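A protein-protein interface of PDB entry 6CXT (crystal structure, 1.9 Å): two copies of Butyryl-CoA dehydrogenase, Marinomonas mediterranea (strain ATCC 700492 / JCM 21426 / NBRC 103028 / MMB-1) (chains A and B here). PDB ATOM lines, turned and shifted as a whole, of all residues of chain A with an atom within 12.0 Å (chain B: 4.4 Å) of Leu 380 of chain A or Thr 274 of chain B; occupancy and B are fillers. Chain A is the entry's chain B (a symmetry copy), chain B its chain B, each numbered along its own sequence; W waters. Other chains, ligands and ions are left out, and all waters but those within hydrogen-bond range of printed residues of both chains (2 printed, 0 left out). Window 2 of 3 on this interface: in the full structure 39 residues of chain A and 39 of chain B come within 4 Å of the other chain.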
ATOM      1  N   ARG A 370       1.683  -1.806 -29.221  1.00  0.00           N
ATOM      2  CA  ARG A 370       2.647  -0.752 -28.888  1.00  0.00           C
ATOM      3  C   ARG A 370       2.093   0.181 -27.806  1.00  0.00           C
ATOM      4  O   ARG A 370       2.863   0.626 -26.961  1.00  0.00           O
ATOM      5  CB  ARG A 370       3.037   0.058 -30.104  1.00  0.00           C
ATOM      6  CG  ARG A 370       3.932  -0.852 -31.033  1.00  0.00           C
ATOM      7  CD  ARG A 370       4.570   0.072 -32.118  1.00  0.00           C
ATOM      8  NE  ARG A 370       5.315  -0.792 -33.082  1.00  0.00           N
ATOM      9  CZ  ARG A 370       4.810  -1.305 -34.223  1.00  0.00           C
ATOM     10  NH1 ARG A 370       3.541  -1.080 -34.596  1.00  0.00           N
ATOM     11  NH2 ARG A 370       5.588  -2.116 -34.976  1.00  0.00           N
ATOM     12  N   GLU A 371       0.786   0.443 -27.839  1.00  0.00           N
ATOM     13  CA  GLU A 371       0.176   1.163 -26.704  1.00  0.00           C
ATOM     14  C   GLU A 371       0.441   0.486 -25.375  1.00  0.00           C
ATOM     15  O   GLU A 371       0.827   1.155 -24.405  1.00  0.00           O
ATOM     16  CB  GLU A 371      -1.335   1.403 -26.898  1.00  0.00           C
ATOM     17  CG  GLU A 371      -1.591   2.435 -27.944  1.00  0.00           C
ATOM     18  CD  GLU A 371      -1.151   3.814 -27.490  1.00  0.00           C
ATOM     19  OE1 GLU A 371      -1.839   4.454 -26.684  1.00  0.00           O
ATOM     20  OE2 GLU A 371      -0.106   4.291 -27.923  1.00  0.00           O
ATOM     21  N   LEU A 372       0.232  -0.824 -25.315  1.00  0.00           N
ATOM     22  CA  LEU A 372       0.510  -1.554 -24.105  1.00  0.00           C
ATOM     23  C   LEU A 372       1.979  -1.555 -23.737  1.00  0.00           C
ATOM     24  O   LEU A 372       2.343  -1.397 -22.582  1.00  0.00           O
ATOM     25  CB  LEU A 372       0.081  -3.017 -24.255  1.00  0.00           C
ATOM     26  CG  LEU A 372      -1.461  -3.092 -24.292  1.00  0.00           C
ATOM     27  CD1 LEU A 372      -1.938  -4.362 -25.038  1.00  0.00           C
ATOM     28  CD2 LEU A 372      -1.917  -3.036 -22.825  1.00  0.00           C
ATOM     29  N   ILE A 373       2.845  -1.796 -24.724  1.00  0.00           N
ATOM     30  CA  ILE A 373       4.286  -1.723 -24.412  1.00  0.00           C
ATOM     31  C   ILE A 373       4.670  -0.336 -23.817  1.00  0.00           C
ATOM     32  O   ILE A 373       5.389  -0.301 -22.814  1.00  0.00           O
ATOM     33  CB  ILE A 373       5.106  -2.030 -25.710  1.00  0.00           C
ATOM     34  CG1 ILE A 373       4.886  -3.511 -26.115  1.00  0.00           C
ATOM     35  CG2 ILE A 373       6.609  -1.761 -25.478  1.00  0.00           C
ATOM     36  CD1 ILE A 373       5.135  -3.784 -27.624  1.00  0.00           C
ATOM     37  N   CYS A 374       4.245   0.742 -24.458  1.00  0.00           N
ATOM     38  CA  CYS A 374       4.546   2.103 -24.035  1.00  0.00           C
ATOM     39  C   CYS A 374       4.075   2.299 -22.586  1.00  0.00           C
ATOM     40  O   CYS A 374       4.835   2.809 -21.749  1.00  0.00           O
ATOM     41  CB  CYS A 374       3.792   3.134 -24.882  1.00  0.00           C
ATOM     42  SG  CYS A 374       4.511   3.241 -26.550  1.00  0.00           S
ATOM     43  N   ASN A 375       2.862   1.804 -22.299  1.00  0.00           N
ATOM     44  CA  ASN A 375       2.341   1.910 -20.941  1.00  0.00           C
ATOM     45  C   ASN A 375       3.219   1.162 -19.928  1.00  0.00           C
ATOM     46  O   ASN A 375       3.614   1.746 -18.886  1.00  0.00           O
ATOM     47  CB  ASN A 375       0.881   1.426 -20.916  1.00  0.00           C
ATOM     48  CG  ASN A 375       0.307   1.407 -19.499  1.00  0.00           C
ATOM     49  OD1 ASN A 375       0.322   0.371 -18.856  1.00  0.00           O
ATOM     50  ND2 ASN A 375      -0.118   2.574 -18.999  1.00  0.00           N
ATOM     51  N   ARG A 376       3.587  -0.095 -20.231  1.00  0.00           N
ATOM     52  CA  ARG A 376       4.458  -0.844 -19.360  1.00  0.00           C
ATOM     53  C   ARG A 376       5.880  -0.310 -19.269  1.00  0.00           C
ATOM     54  O   ARG A 376       6.573  -0.579 -18.294  1.00  0.00           O
ATOM     55  CB  ARG A 376       4.464  -2.359 -19.697  1.00  0.00           C
ATOM     56  CG  ARG A 376       3.130  -3.050 -19.520  1.00  0.00           C
ATOM     57  CD  ARG A 376       2.515  -2.730 -18.124  1.00  0.00           C
ATOM     58  NE  ARG A 376       1.340  -3.561 -17.817  1.00  0.00           N
ATOM     59  CZ  ARG A 376       0.094  -3.420 -18.286  1.00  0.00           C
ATOM     60  NH1 ARG A 376      -0.240  -2.466 -19.157  1.00  0.00           N
ATOM     61  NH2 ARG A 376      -0.853  -4.289 -17.863  1.00  0.00           N
ATOM     62  N   LEU A 377       6.317   0.470 -20.255  1.00  0.00           N
ATOM     63  CA  LEU A 377       7.617   1.146 -20.145  1.00  0.00           C
ATOM     64  C   LEU A 377       7.494   2.365 -19.239  1.00  0.00           C
ATOM     65  O   LEU A 377       8.506   2.955 -18.858  1.00  0.00           O
ATOM     66  CB  LEU A 377       8.118   1.583 -21.538  1.00  0.00           C
ATOM     67  CG  LEU A 377       8.523   0.438 -22.493  1.00  0.00           C
ATOM     68  CD1 LEU A 377       8.928   1.053 -23.872  1.00  0.00           C
ATOM     69  CD2 LEU A 377       9.742  -0.327 -21.973  1.00  0.00           C
ATOM     70  N   GLY A 378       6.262   2.766 -18.921  1.00  0.00           N
ATOM     71  CA  GLY A 378       6.057   3.910 -18.028  1.00  0.00           C
ATOM     72  C   GLY A 378       5.865   5.219 -18.767  1.00  0.00           C
ATOM     73  O   GLY A 378       5.909   6.291 -18.134  1.00  0.00           O
ATOM     74  N   LEU A 379       5.657   5.170 -20.100  1.00  0.00           N
ATOM     75  CA  LEU A 379       5.386   6.364 -20.874  1.00  0.00           C
ATOM     76  C   LEU A 379       4.038   6.950 -20.552  1.00  0.00           C
ATOM     77  O   LEU A 379       3.023   6.228 -20.571  1.00  0.00           O
ATOM     78  CB  LEU A 379       5.495   6.130 -22.425  1.00  0.00           C
ATOM     79  CG  LEU A 379       6.976   5.892 -22.890  1.00  0.00           C
ATOM     80  CD1 LEU A 379       7.003   5.175 -24.258  1.00  0.00           C
ATOM     81  CD2 LEU A 379       7.813   7.175 -22.936  1.00  0.00           C
ATOM     82  N   LEU A 380       4.032   8.259 -20.311  1.00  0.00           N
ATOM     83  CA  LEU A 380       2.798   8.941 -19.936  1.00  0.00           C
ATOM     84  C   LEU A 380       1.879   9.176 -21.117  1.00  0.00           C
ATOM     85  O   LEU A 380       0.631   9.081 -21.006  1.00  0.00           O
ATOM     86  CB  LEU A 380       3.149  10.296 -19.281  1.00  0.00           C
ATOM     87  CG  LEU A 380       3.963  10.179 -17.992  1.00  0.00           C
ATOM     88  CD1 LEU A 380       4.093  11.614 -17.480  1.00  0.00           C
ATOM     89  CD2 LEU A 380       3.332   9.231 -16.941  1.00  0.00           C
ATOM     90  OXT LEU A 380       2.339   9.494 -22.219  1.00  0.00           O
ATOM     91  N   ALA B 265      10.991  11.655 -22.839  1.00  0.00           N
ATOM     92  CA  ALA B 265       9.694  11.800 -23.453  1.00  0.00           C
ATOM     93  C   ALA B 265       8.638  12.049 -22.340  1.00  0.00           C
ATOM     94  O   ALA B 265       7.610  12.574 -22.650  1.00  0.00           O
ATOM     95  CB  ALA B 265       9.322  10.553 -24.260  1.00  0.00           C
ATOM     96  N   ASN B 266       8.916  11.635 -21.107  1.00  0.00           N
ATOM     97  CA  ASN B 266       7.978  11.886 -19.959  1.00  0.00           C
ATOM     98  C   ASN B 266       8.184  13.260 -19.327  1.00  0.00           C
ATOM     99  O   ASN B 266       7.365  13.681 -18.516  1.00  0.00           O
ATOM    100  CB  ASN B 266       8.132  10.828 -18.878  1.00  0.00           C
ATOM    101  CG  ASN B 266       7.442   9.526 -19.229  1.00  0.00           C
ATOM    102  OD1 ASN B 266       6.607   9.476 -20.100  1.00  0.00           O
ATOM    103  ND2 ASN B 266       7.791   8.474 -18.530  1.00  0.00           N
ATOM    104  N   ARG B 268       9.858  16.125 -21.289  1.00  0.00           N
ATOM    105  CA  ARG B 268       9.786  17.180 -22.273  1.00  0.00           C
ATOM    106  C   ARG B 268       8.363  17.376 -22.758  1.00  0.00           C
ATOM    107  O   ARG B 268       7.708  16.430 -23.188  1.00  0.00           O
ATOM    108  CB  ARG B 268      10.725  16.896 -23.483  1.00  0.00           C
ATOM    109  CG  ARG B 268      10.434  17.704 -24.745  1.00  0.00           C
ATOM    110  CD  ARG B 268      11.068  19.070 -24.567  1.00  0.00           C
ATOM    111  NE  ARG B 268      11.218  19.884 -25.787  1.00  0.00           N
ATOM    112  CZ  ARG B 268      11.699  21.133 -25.747  1.00  0.00           C
ATOM    113  NH1 ARG B 268      12.021  21.681 -24.556  1.00  0.00           N
ATOM    114  NH2 ARG B 268      11.902  21.846 -26.852  1.00  0.00           N
ATOM    115  N   MET B 269       7.922  18.639 -22.761  1.00  0.00           N
ATOM    116  CA  MET B 269       6.601  18.986 -23.202  1.00  0.00           C
ATOM    117  C   MET B 269       6.656  19.842 -24.432  1.00  0.00           C
ATOM    118  O   MET B 269       7.560  20.665 -24.587  1.00  0.00           O
ATOM    119  CB  MET B 269       5.842  19.718 -22.071  1.00  0.00           C
ATOM    120  CG  MET B 269       5.498  18.790 -20.915  1.00  0.00           C
ATOM    121  SD  MET B 269       4.648  19.605 -19.561  1.00  0.00           S
ATOM    122  CE  MET B 269       2.967  19.726 -20.187  1.00  0.00           C
ATOM    123  N   LYS B 273       1.510  19.120 -23.459  1.00  0.00           N
ATOM    124  CA  LYS B 273       1.566  17.684 -23.144  1.00  0.00           C
ATOM    125  C   LYS B 273       3.007  17.155 -23.212  1.00  0.00           C
ATOM    126  O   LYS B 273       3.800  17.706 -23.944  1.00  0.00           O
ATOM    127  CB  LYS B 273       0.644  16.881 -24.062  1.00  0.00           C
ATOM    128  CG  LYS B 273       0.900  17.057 -25.549  1.00  0.00           C
ATOM    129  CD  LYS B 273      -0.396  16.969 -26.336  1.00  0.00           C
ATOM    130  CE  LYS B 273      -0.600  15.590 -26.916  1.00  0.00           C
ATOM    131  NZ  LYS B 273      -1.967  15.496 -27.494  1.00  0.00           N
ATOM    132  N   THR B 274       3.324  16.091 -22.487  1.00  0.00           N
ATOM    133  CA  THR B 274       4.621  15.437 -22.663  1.00  0.00           C
ATOM    134  C   THR B 274       4.688  14.848 -24.098  1.00  0.00           C
ATOM    135  O   THR B 274       3.669  14.444 -24.668  1.00  0.00           O
ATOM    136  CB  THR B 274       4.831  14.350 -21.630  1.00  0.00           C
ATOM    137  OG1 THR B 274       3.749  13.391 -21.717  1.00  0.00           O
ATOM    138  CG2 THR B 274       4.828  15.013 -20.243  1.00  0.00           C
ATOM    139  N   ILE B 275       5.881  14.807 -24.682  1.00  0.00           N
ATOM    140  CA  ILE B 275       5.989  14.323 -26.075  1.00  0.00           C
ATOM    141  C   ILE B 275       5.657  12.837 -26.147  1.00  0.00           C
ATOM    142  O   ILE B 275       5.342  12.315 -27.242  1.00  0.00           O
ATOM    143  CB  ILE B 275       7.384  14.631 -26.677  1.00  0.00           C
ATOM    144  CG1 ILE B 275       8.516  13.984 -25.828  1.00  0.00           C
ATOM    145  CG2 ILE B 275       7.522  16.157 -26.838  1.00  0.00           C
ATOM    146  CD1 ILE B 275       9.906  14.058 -26.524  1.00  0.00           C
ATOM    147  N   SER B 276       5.717  12.165 -25.012  1.00  0.00           N
ATOM    148  CA  SER B 276       5.237  10.751 -24.859  1.00  0.00           C
ATOM    149  C   SER B 276       3.797  10.566 -25.304  1.00  0.00           C
ATOM    150  O   SER B 276       3.368   9.452 -25.582  1.00  0.00           O
ATOM    151  CB  SER B 276       5.391  10.235 -23.421  1.00  0.00           C
ATOM    152  OG  SER B 276       4.421  10.913 -22.596  1.00  0.00           O
ATOM    153  N   ARG B 277       3.045  11.666 -25.377  1.00  0.00           N
ATOM    154  CA  ARG B 277       1.657  11.550 -25.775  1.00  0.00           C
ATOM    155  C   ARG B 277       1.501  11.507 -27.300  1.00  0.00           C
ATOM    156  O   ARG B 277       0.412  11.251 -27.799  1.00  0.00           O
ATOM    157  CB  ARG B 277       0.859  12.738 -25.193  1.00  0.00           C
ATOM    158  CG  ARG B 277       0.572  12.610 -23.700  1.00  0.00           C
ATOM    159  CD  ARG B 277      -0.456  11.488 -23.518  1.00  0.00           C
ATOM    160  NE  ARG B 277      -0.901  11.292 -22.143  1.00  0.00           N
ATOM    161  CZ  ARG B 277      -1.789  12.054 -21.476  1.00  0.00           C
ATOM    162  NH1 ARG B 277      -2.361  13.122 -22.035  1.00  0.00           N
ATOM    163  NH2 ARG B 277      -2.102  11.723 -20.218  1.00  0.00           N
HETATM  164  O   HOH W   1      -0.973   9.386 -18.791  1.00  0.00           O
HETATM  165  O   HOH W   2       1.666   7.546 -24.423  1.00  0.00           O
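Water W1 lies within hydrogen-bond range of the chain-end carboxylate (O) of Leu 380 of chain A and the guanidinium group (NH2) of Arg 277 of chain B.
Water W2 bridges the backbone carbonyl oxygen of Ser 276 of chain B (2.8 Å) and the chain-end carboxylate of Leu 380 of chain A (3.0 Å).
Of the 11 printed residues of chain A, 3 touch a printed residue of chain B.
Printed residues of chain A that touch a printed residue of chain B: Gly 378, Leu 379 and Leu 380.
Of the 9 printed residues of chain B, 5 touch a printed residue of chain A.
Printed residues of chain B that touch a printed residue of chain A: Ala 265, Asn 266, Thr 274, Ser 276 and Arg 277.
Hydrophobic or aromatic side chains of chain B that line the printed part of chain A: Ala 265.
Among the printed residues, 8 pairs touch across the chains.
The backbone carbonyl oxygen (O) of Gly 378 of chain A is in hydrogen-bond range of the side-chain amide nitrogen (ND2) of Asn 266 of chain B (2.9 Å).
The guanidinium group (NE) of Arg 277 of chain B lies within salt-bridge range of the chain-end carboxylate (O) of Leu 380 of chain A.
OG of Ser 276 of chain B is in hydrogen-bond range of OXT of Leu 380 of chain A (2.5 Å).
The side-chain amide oxygen of Asn 266 of chain B lies within hydrogen-bond range of the backbone NH of Leu 380 of chain A, 2.9 Å away.
Leu 379 of chain A touches Ala 265 of chain B (CD2 to CB, 3.9 Å).
CA of Leu 379 of chain A touches OD1 of Asn 266 of chain B (3.4 Å).
Leu 379 of chain A touches Ser 276 of chain B.
Thr 274 of chain B touches Leu 380 of chain A.
Of the printed residues of chain B, Leu 380 of chain A touches Asn 266, Thr 274, Ser 276 and Arg 277.
Of the printed residues of chain A, Thr 274 of chain B touches Leu 380 (3.98 Å).
Asn 266 of chain B touches just these residues of chain A: Gly 378, Leu 379 and Leu 380.
No residue of chain A comes within 4 Å of Met 269 of chain B.
No residue of chain A comes within 4 Å of Ile 275 of chain B.
Of the printed residues of chain A, Arg 277 of chain B touches Leu 380.
Of the printed residues of chain B, Gly 378 of chain A touches Asn 266 (2.9 Å).
Printed residues of chain B within 4 Å of Leu 379 of chain A: Ala 265, Asn 266 and Ser 276.
Leu 372 of chain A touches none of the printed residues of chain B.
Leu 377 of chain A touches none of the printed residues of chain B.
The nearest printed residue of chain B that does not touch Leu 380 of chain A is Ala 265 of chain B (6.0 Å).
The nearest printed residue of chain A that does not touch Thr 274 of chain B is Leu 379 of chain A (6.6 Å).
O of Ala 265 of chain B sits at hydrogen-bond distance from N of Ile 275 of chain B (3.5 Å).
N of Ser 276 of chain B lies within hydrogen-bond range of O of Ala 265 of chain B (3.1 Å).
O of Cys 374 of chain A lies within hydrogen-bond range of N of Leu 379 of chain A (3.0 Å).
The side-chain hydroxyl (OG1) of Thr 274 of chain B lies within hydrogen-bond range of the side-chain hydroxyl (OG) of Ser 276 of chain B (2.7 Å).
No position is printed for both chains.
Of the 8 pairs that touch across the chains among the printed residues, none has its exchanged pair printed and touching as well.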
